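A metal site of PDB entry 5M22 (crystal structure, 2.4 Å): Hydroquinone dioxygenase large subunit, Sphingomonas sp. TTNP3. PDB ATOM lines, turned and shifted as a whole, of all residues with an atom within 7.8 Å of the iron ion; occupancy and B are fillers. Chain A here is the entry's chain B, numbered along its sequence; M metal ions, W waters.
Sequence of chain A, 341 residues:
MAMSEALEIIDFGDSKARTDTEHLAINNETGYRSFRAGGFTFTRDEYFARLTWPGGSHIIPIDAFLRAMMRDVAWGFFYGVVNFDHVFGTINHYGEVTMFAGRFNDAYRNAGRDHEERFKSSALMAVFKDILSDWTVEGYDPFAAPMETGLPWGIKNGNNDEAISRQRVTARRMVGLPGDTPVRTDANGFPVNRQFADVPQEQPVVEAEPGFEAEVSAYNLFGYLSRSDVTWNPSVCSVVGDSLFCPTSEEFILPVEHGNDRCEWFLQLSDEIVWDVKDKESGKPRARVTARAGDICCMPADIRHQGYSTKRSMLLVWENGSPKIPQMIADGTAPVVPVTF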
ATOM      1  N   TRP A  75      19.347   8.808  23.624  1.00  0.00           N
ATOM      2  CA  TRP A  75      19.723   8.402  24.996  1.00  0.00           C
ATOM      3  C   TRP A  75      20.972   9.120  25.516  1.00  0.00           C
ATOM      4  O   TRP A  75      21.433   8.841  26.620  1.00  0.00           O
ATOM      5  CB  TRP A  75      19.944   6.891  25.120  1.00  0.00           C
ATOM      6  CG  TRP A  75      18.775   5.997  24.785  1.00  0.00           C
ATOM      7  CD1 TRP A  75      17.431   6.312  24.827  1.00  0.00           C
ATOM      8  CD2 TRP A  75      18.840   4.621  24.387  1.00  0.00           C
ATOM      9  NE1 TRP A  75      16.667   5.232  24.455  1.00  0.00           N
ATOM     10  CE2 TRP A  75      17.504   4.178  24.189  1.00  0.00           C
ATOM     11  CE3 TRP A  75      19.893   3.720  24.173  1.00  0.00           C
ATOM     12  CZ2 TRP A  75      17.201   2.856  23.782  1.00  0.00           C
ATOM     13  CZ3 TRP A  75      19.594   2.420  23.763  1.00  0.00           C
ATOM     14  CH2 TRP A  75      18.256   2.003  23.583  1.00  0.00           C
ATOM     15  N   PHE A  78      23.596   6.821  26.581  1.00  0.00           N
ATOM     16  CA  PHE A  78      23.022   5.831  27.517  1.00  0.00           C
ATOM     17  C   PHE A  78      23.920   5.478  28.707  1.00  0.00           C
ATOM     18  O   PHE A  78      24.664   6.319  29.179  1.00  0.00           O
ATOM     19  CB  PHE A  78      22.519   4.596  26.754  1.00  0.00           C
ATOM     20  CG  PHE A  78      21.373   3.873  27.432  1.00  0.00           C
ATOM     21  CD1 PHE A  78      20.382   4.573  28.136  1.00  0.00           C
ATOM     22  CD2 PHE A  78      21.236   2.490  27.329  1.00  0.00           C
ATOM     23  CE1 PHE A  78      19.309   3.909  28.734  1.00  0.00           C
ATOM     24  CE2 PHE A  78      20.166   1.833  27.922  1.00  0.00           C
ATOM     25  CZ  PHE A  78      19.206   2.538  28.629  1.00  0.00           C
ATOM     26  N   TYR A  79      23.821   4.267  29.241  1.00  0.00           N
ATOM     27  CA  TYR A  79      24.776   3.817  30.263  1.00  0.00           C
ATOM     28  C   TYR A  79      25.651   2.764  29.611  1.00  0.00           C
ATOM     29  O   TYR A  79      25.155   1.930  28.867  1.00  0.00           O
ATOM     30  CB  TYR A  79      24.074   3.211  31.493  1.00  0.00           C
ATOM     31  CG  TYR A  79      23.285   4.209  32.290  1.00  0.00           C
ATOM     32  CD1 TYR A  79      23.930   5.089  33.156  1.00  0.00           C
ATOM     33  CD2 TYR A  79      21.906   4.291  32.159  1.00  0.00           C
ATOM     34  CE1 TYR A  79      23.223   6.038  33.866  1.00  0.00           C
ATOM     35  CE2 TYR A  79      21.177   5.235  32.869  1.00  0.00           C
ATOM     36  CZ  TYR A  79      21.845   6.100  33.724  1.00  0.00           C
ATOM     37  OH  TYR A  79      21.137   7.035  34.431  1.00  0.00           O
ATOM     38  N   VAL A  81      27.896   0.405  27.392  1.00  0.00           N
ATOM     39  CA  VAL A  81      28.157   0.060  25.969  1.00  0.00           C
ATOM     40  C   VAL A  81      26.880  -0.019  25.194  1.00  0.00           C
ATOM     41  O   VAL A  81      25.987  -0.788  25.562  1.00  0.00           O
ATOM     42  CB  VAL A  81      28.859  -1.304  25.845  1.00  0.00           C
ATOM     43  CG1 VAL A  81      29.281  -1.554  24.382  1.00  0.00           C
ATOM     44  CG2 VAL A  81      30.043  -1.378  26.793  1.00  0.00           C
ATOM     45  N   PRO A 234      13.534   4.089  27.333  1.00  0.00           N
ATOM     46  CA  PRO A 234      13.387   4.234  28.776  1.00  0.00           C
ATOM     47  C   PRO A 234      13.363   5.725  29.160  1.00  0.00           C
ATOM     48  O   PRO A 234      14.157   6.509  28.710  1.00  0.00           O
ATOM     49  CB  PRO A 234      14.651   3.549  29.312  1.00  0.00           C
ATOM     50  CG  PRO A 234      14.938   2.495  28.298  1.00  0.00           C
ATOM     51  CD  PRO A 234      14.690   3.223  27.000  1.00  0.00           C
ATOM     52  N   LEU A 254      14.811  -4.495  20.179  1.00  0.00           N
ATOM     53  CA  LEU A 254      15.666  -3.448  20.693  1.00  0.00           C
ATOM     54  C   LEU A 254      16.772  -3.214  19.666  1.00  0.00           C
ATOM     55  O   LEU A 254      17.463  -4.140  19.276  1.00  0.00           O
ATOM     56  CB  LEU A 254      16.237  -3.805  22.066  1.00  0.00           C
ATOM     57  CG  LEU A 254      17.123  -2.738  22.698  1.00  0.00           C
ATOM     58  CD1 LEU A 254      16.367  -1.473  23.074  1.00  0.00           C
ATOM     59  CD2 LEU A 254      17.849  -3.271  23.928  1.00  0.00           C
ATOM     60  N   VAL A 256      19.622  -2.160  19.604  1.00  0.00           N
ATOM     61  CA  VAL A 256      21.013  -2.242  20.054  1.00  0.00           C
ATOM     62  C   VAL A 256      21.153  -3.439  21.001  1.00  0.00           C
ATOM     63  O   VAL A 256      20.146  -3.917  21.535  1.00  0.00           O
ATOM     64  CB  VAL A 256      21.443  -0.937  20.775  1.00  0.00           C
ATOM     65  CG1 VAL A 256      21.083   0.293  19.952  1.00  0.00           C
ATOM     66  CG2 VAL A 256      20.795  -0.852  22.143  1.00  0.00           C
ATOM     67  N   GLU A 257      22.381  -3.933  21.173  1.00  0.00           N
ATOM     68  CA  GLU A 257      22.749  -4.863  22.253  1.00  0.00           C
ATOM     69  C   GLU A 257      23.384  -4.037  23.384  1.00  0.00           C
ATOM     70  O   GLU A 257      24.498  -3.511  23.227  1.00  0.00           O
ATOM     71  CB  GLU A 257      23.722  -5.958  21.753  1.00  0.00           C
ATOM     72  CG  GLU A 257      23.245  -6.752  20.527  1.00  0.00           C
ATOM     73  CD  GLU A 257      24.121  -7.958  20.167  1.00  0.00           C
ATOM     74  OE1 GLU A 257      25.368  -7.920  20.336  1.00  0.00           O
ATOM     75  OE2 GLU A 257      23.572  -8.974  19.700  1.00  0.00           O
ATOM     76  N   HIS A 258      22.676  -3.910  24.508  1.00  0.00           N
ATOM     77  CA  HIS A 258      23.114  -3.035  25.615  1.00  0.00           C
ATOM     78  C   HIS A 258      23.972  -3.762  26.624  1.00  0.00           C
ATOM     79  O   HIS A 258      23.492  -4.646  27.321  1.00  0.00           O
ATOM     80  CB  HIS A 258      21.913  -2.417  26.316  1.00  0.00           C
ATOM     81  CG  HIS A 258      22.272  -1.537  27.481  1.00  0.00           C
ATOM     82  ND1 HIS A 258      21.456  -1.385  28.590  1.00  0.00           N
ATOM     83  CD2 HIS A 258      23.359  -0.756  27.721  1.00  0.00           C
ATOM     84  CE1 HIS A 258      22.010  -0.543  29.429  1.00  0.00           C
ATOM     85  NE2 HIS A 258      23.163  -0.149  28.934  1.00  0.00           N
ATOM     86  N   GLY A 259      25.250  -3.400  26.695  1.00  0.00           N
ATOM     87  CA  GLY A 259      26.161  -3.913  27.731  1.00  0.00           C
ATOM     88  C   GLY A 259      26.340  -2.844  28.809  1.00  0.00           C
ATOM     89  O   GLY A 259      27.165  -1.931  28.710  1.00  0.00           O
ATOM     90  N   ASN A 260      25.524  -2.931  29.844  1.00  0.00           N
ATOM     91  CA  ASN A 260      25.550  -1.915  30.882  1.00  0.00           C
ATOM     92  C   ASN A 260      26.822  -2.003  31.705  1.00  0.00           C
ATOM     93  O   ASN A 260      27.404  -3.077  31.836  1.00  0.00           O
ATOM     94  CB  ASN A 260      24.332  -2.034  31.765  1.00  0.00           C
ATOM     95  CG  ASN A 260      23.833  -0.692  32.233  1.00  0.00           C
ATOM     96  OD1 ASN A 260      24.634   0.260  32.379  1.00  0.00           O
ATOM     97  ND2 ASN A 260      22.531  -0.593  32.494  1.00  0.00           N
ATOM     98  N   ARG A 262      26.758  -1.495  34.913  1.00  0.00           N
ATOM     99  CA  ARG A 262      26.047  -1.545  36.181  1.00  0.00           C
ATOM    100  C   ARG A 262      24.919  -2.591  36.030  1.00  0.00           C
ATOM    101  O   ARG A 262      24.562  -2.954  34.921  1.00  0.00           O
ATOM    102  CB  ARG A 262      25.462  -0.172  36.559  1.00  0.00           C
ATOM    103  CG  ARG A 262      24.329   0.307  35.659  1.00  0.00           C
ATOM    104  CD  ARG A 262      24.104   1.794  35.792  1.00  0.00           C
ATOM    105  NE  ARG A 262      25.309   2.496  35.368  1.00  0.00           N
ATOM    106  CZ  ARG A 262      25.794   3.604  35.919  1.00  0.00           C
ATOM    107  NH1 ARG A 262      25.177   4.200  36.910  1.00  0.00           N
ATOM    108  NH2 ARG A 262      26.918   4.114  35.433  1.00  0.00           N
ATOM    109  N   GLU A 264      21.099  -3.779  36.009  1.00  0.00           N
ATOM    110  CA  GLU A 264      19.806  -3.126  35.706  1.00  0.00           C
ATOM    111  C   GLU A 264      18.710  -4.175  35.843  1.00  0.00           C
ATOM    112  O   GLU A 264      18.953  -5.377  35.638  1.00  0.00           O
ATOM    113  CB  GLU A 264      19.813  -2.371  34.334  1.00  0.00           C
ATOM    114  CG  GLU A 264      19.698  -3.191  33.044  1.00  0.00           C
ATOM    115  CD  GLU A 264      19.580  -2.358  31.742  1.00  0.00           C
ATOM    116  OE1 GLU A 264      19.421  -1.139  31.773  1.00  0.00           O
ATOM    117  OE2 GLU A 264      19.629  -2.913  30.626  1.00  0.00           O
ATOM    118  N   TRP A 265      17.526  -3.732  36.223  1.00  0.00           N
ATOM    119  CA  TRP A 265      16.370  -4.615  36.463  1.00  0.00           C
ATOM    120  C   TRP A 265      15.252  -4.307  35.466  1.00  0.00           C
ATOM    121  O   TRP A 265      15.044  -3.142  35.137  1.00  0.00           O
ATOM    122  CB  TRP A 265      15.850  -4.412  37.880  1.00  0.00           C
ATOM    123  CG  TRP A 265      16.777  -4.956  38.917  1.00  0.00           C
ATOM    124  CD1 TRP A 265      17.925  -4.368  39.400  1.00  0.00           C
ATOM    125  CD2 TRP A 265      16.648  -6.214  39.606  1.00  0.00           C
ATOM    126  NE1 TRP A 265      18.505  -5.183  40.347  1.00  0.00           N
ATOM    127  CE2 TRP A 265      17.755  -6.326  40.479  1.00  0.00           C
ATOM    128  CE3 TRP A 265      15.710  -7.265  39.559  1.00  0.00           C
ATOM    129  CZ2 TRP A 265      17.933  -7.431  41.302  1.00  0.00           C
ATOM    130  CZ3 TRP A 265      15.906  -8.367  40.395  1.00  0.00           C
ATOM    131  CH2 TRP A 265      17.004  -8.445  41.241  1.00  0.00           C
ATOM    132  N   PHE A 266      14.557  -5.344  35.025  1.00  0.00           N
ATOM    133  CA  PHE A 266      13.438  -5.240  34.079  1.00  0.00           C
ATOM    134  C   PHE A 266      12.224  -5.783  34.787  1.00  0.00           C
ATOM    135  O   PHE A 266      12.302  -6.869  35.387  1.00  0.00           O
ATOM    136  CB  PHE A 266      13.659  -6.170  32.884  1.00  0.00           C
ATOM    137  CG  PHE A 266      14.743  -5.737  31.918  1.00  0.00           C
ATOM    138  CD1 PHE A 266      15.092  -4.387  31.783  1.00  0.00           C
ATOM    139  CD2 PHE A 266      15.373  -6.671  31.119  1.00  0.00           C
ATOM    140  CE1 PHE A 266      16.083  -4.004  30.862  1.00  0.00           C
ATOM    141  CE2 PHE A 266      16.340  -6.281  30.214  1.00  0.00           C
ATOM    142  CZ  PHE A 266      16.711  -4.965  30.095  1.00  0.00           C
ATOM    143  N   TRP A 275      14.448 -11.761  26.063  1.00  0.00           N
ATOM    144  CA  TRP A 275      15.724 -11.109  26.132  1.00  0.00           C
ATOM    145  C   TRP A 275      16.767 -12.080  25.628  1.00  0.00           C
ATOM    146  O   TRP A 275      17.016 -13.132  26.234  1.00  0.00           O
ATOM    147  CB  TRP A 275      16.004 -10.663  27.581  1.00  0.00           C
ATOM    148  CG  TRP A 275      15.081  -9.562  27.985  1.00  0.00           C
ATOM    149  CD1 TRP A 275      13.956  -9.660  28.743  1.00  0.00           C
ATOM    150  CD2 TRP A 275      15.181  -8.189  27.596  1.00  0.00           C
ATOM    151  NE1 TRP A 275      13.349  -8.436  28.875  1.00  0.00           N
ATOM    152  CE2 TRP A 275      14.069  -7.519  28.161  1.00  0.00           C
ATOM    153  CE3 TRP A 275      16.105  -7.478  26.809  1.00  0.00           C
ATOM    154  CZ2 TRP A 275      13.865  -6.151  27.983  1.00  0.00           C
ATOM    155  CZ3 TRP A 275      15.893  -6.135  26.611  1.00  0.00           C
ATOM    156  CH2 TRP A 275      14.770  -5.477  27.207  1.00  0.00           C
ATOM    157  N   MET A 299      19.616  -7.904  35.026  1.00  0.00           N
ATOM    158  CA  MET A 299      20.633  -8.069  34.015  1.00  0.00           C
ATOM    159  C   MET A 299      21.976  -7.792  34.655  1.00  0.00           C
ATOM    160  O   MET A 299      22.272  -6.646  35.003  1.00  0.00           O
ATOM    161  CB  MET A 299      20.405  -7.110  32.826  1.00  0.00           C
ATOM    162  CG  MET A 299      19.221  -7.431  31.908  1.00  0.00           C
ATOM    163  SD  MET A 299      19.343  -8.976  30.978  1.00  0.00           S
ATOM    164  CE  MET A 299      17.705  -9.637  31.213  1.00  0.00           C
ATOM    165  N   ILE A 303      26.959  -8.872  31.161  1.00  0.00           N
ATOM    166  CA  ILE A 303      26.237  -9.306  29.973  1.00  0.00           C
ATOM    167  C   ILE A 303      25.785  -8.135  29.075  1.00  0.00           C
ATOM    168  O   ILE A 303      25.696  -6.996  29.519  1.00  0.00           O
ATOM    169  CB  ILE A 303      25.066 -10.274  30.300  1.00  0.00           C
ATOM    170  CG1 ILE A 303      23.957  -9.623  31.131  1.00  0.00           C
ATOM    171  CG2 ILE A 303      25.580 -11.507  31.028  1.00  0.00           C
ATOM    172  CD1 ILE A 303      22.838  -8.996  30.325  1.00  0.00           C
ATOM    173  N   ARG A 304      25.523  -8.436  27.811  1.00  0.00           N
ATOM    174  CA  ARG A 304      24.790  -7.505  26.938  1.00  0.00           C
ATOM    175  C   ARG A 304      23.435  -8.151  26.673  1.00  0.00           C
ATOM    176  O   ARG A 304      23.284  -9.386  26.761  1.00  0.00           O
ATOM    177  CB  ARG A 304      25.548  -7.271  25.631  1.00  0.00           C
ATOM    178  CG  ARG A 304      25.635  -8.486  24.725  1.00  0.00           C
ATOM    179  CD  ARG A 304      26.283  -8.162  23.367  1.00  0.00           C
ATOM    180  NE  ARG A 304      27.719  -8.067  23.528  1.00  0.00           N
ATOM    181  CZ  ARG A 304      28.621  -7.991  22.556  1.00  0.00           C
ATOM    182  NH1 ARG A 304      28.253  -8.014  21.278  1.00  0.00           N
ATOM    183  NH2 ARG A 304      29.904  -7.911  22.877  1.00  0.00           N
ATOM    184  N   HIS A 305      22.429  -7.339  26.357  1.00  0.00           N
ATOM    185  CA  HIS A 305      21.088  -7.891  26.163  1.00  0.00           C
ATOM    186  C   HIS A 305      20.349  -7.179  25.024  1.00  0.00           C
ATOM    187  O   HIS A 305      20.591  -5.990  24.748  1.00  0.00           O
ATOM    188  CB  HIS A 305      20.282  -7.763  27.443  1.00  0.00           C
ATOM    189  CG  HIS A 305      20.398  -6.415  28.073  1.00  0.00           C
ATOM    190  ND1 HIS A 305      21.307  -6.119  29.059  1.00  0.00           N
ATOM    191  CD2 HIS A 305      19.752  -5.253  27.802  1.00  0.00           C
ATOM    192  CE1 HIS A 305      21.204  -4.851  29.392  1.00  0.00           C
ATOM    193  NE2 HIS A 305      20.269  -4.299  28.639  1.00  0.00           N
ATOM    194  N   GLN A 306      19.432  -7.914  24.403  1.00  0.00           N
ATOM    195  CA  GLN A 306      18.576  -7.397  23.325  1.00  0.00           C
ATOM    196  C   GLN A 306      17.182  -8.093  23.317  1.00  0.00           C
ATOM    197  O   GLN A 306      17.102  -9.318  23.233  1.00  0.00           O
ATOM    198  CB  GLN A 306      19.297  -7.573  21.988  1.00  0.00           C
ATOM    199  CG  GLN A 306      18.528  -7.144  20.752  1.00  0.00           C
ATOM    200  CD  GLN A 306      19.376  -7.261  19.509  1.00  0.00           C
ATOM    201  OE1 GLN A 306      19.957  -8.304  19.262  1.00  0.00           O
ATOM    202  NE2 GLN A 306      19.466  -6.178  18.729  1.00  0.00           N
ATOM    203  N   VAL A 317      12.069  -0.431  33.053  1.00  0.00           N
ATOM    204  CA  VAL A 317      13.512  -0.510  33.182  1.00  0.00           C
ATOM    205  C   VAL A 317      13.836   0.266  34.456  1.00  0.00           C
ATOM    206  O   VAL A 317      13.417   1.417  34.628  1.00  0.00           O
ATOM    207  CB  VAL A 317      14.243   0.126  31.972  1.00  0.00           C
ATOM    208  CG1 VAL A 317      15.735  -0.078  32.091  1.00  0.00           C
ATOM    209  CG2 VAL A 317      13.754  -0.485  30.658  1.00  0.00           C
ATOM    210  N   GLU A 319      16.805   1.673  36.969  1.00  0.00           N
ATOM    211  CA  GLU A 319      18.232   1.992  37.012  1.00  0.00           C
ATOM    212  C   GLU A 319      18.713   2.599  38.354  1.00  0.00           C
ATOM    213  O   GLU A 319      17.999   3.372  39.005  1.00  0.00           O
ATOM    214  CB  GLU A 319      18.614   2.978  35.904  1.00  0.00           C
ATOM    215  CG  GLU A 319      18.225   2.638  34.482  1.00  0.00           C
ATOM    216  CD  GLU A 319      19.201   1.698  33.752  1.00  0.00           C
ATOM    217  OE1 GLU A 319      20.334   1.356  34.247  1.00  0.00           O
ATOM    218  OE2 GLU A 319      18.829   1.319  32.614  1.00  0.00           O
HETATM  219 FE    FE M   1      19.683  -2.307  29.021  1.00  0.00          FE
HETATM  220  O   HOH W   1      17.827  -1.433  27.866  1.00  0.00           O
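Three residues have an atom within 4 Å of the iron ion: His 258, Glu 264 and His 305.
The backbone carbonyl oxygen (O) of Glu 264 sits at hydrogen-bond distance from the backbone NH (N) of Met 299 (2.7 Å).
The side-chain carboxylate of Glu 264 sits close to the side-chain carboxylate of Glu 319, at 2.7 Å.
The side-chain carboxylate (OE1) of Glu 264 is in hydrogen-bond range of the side-chain amide nitrogen (ND2) of Asn 260, 3.2 Å away.
The backbone carbonyl oxygen (O) of Tyr 79 lies within hydrogen-bond range of a ring nitrogen (NE2) of His 258.
The iron ion is bound by OE2 of Glu 264 (1.7 Å), ND1 of His 258 (2.0 Å), NE2 of His 305 (2.1 Å) and water W1 (2.4 Å).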
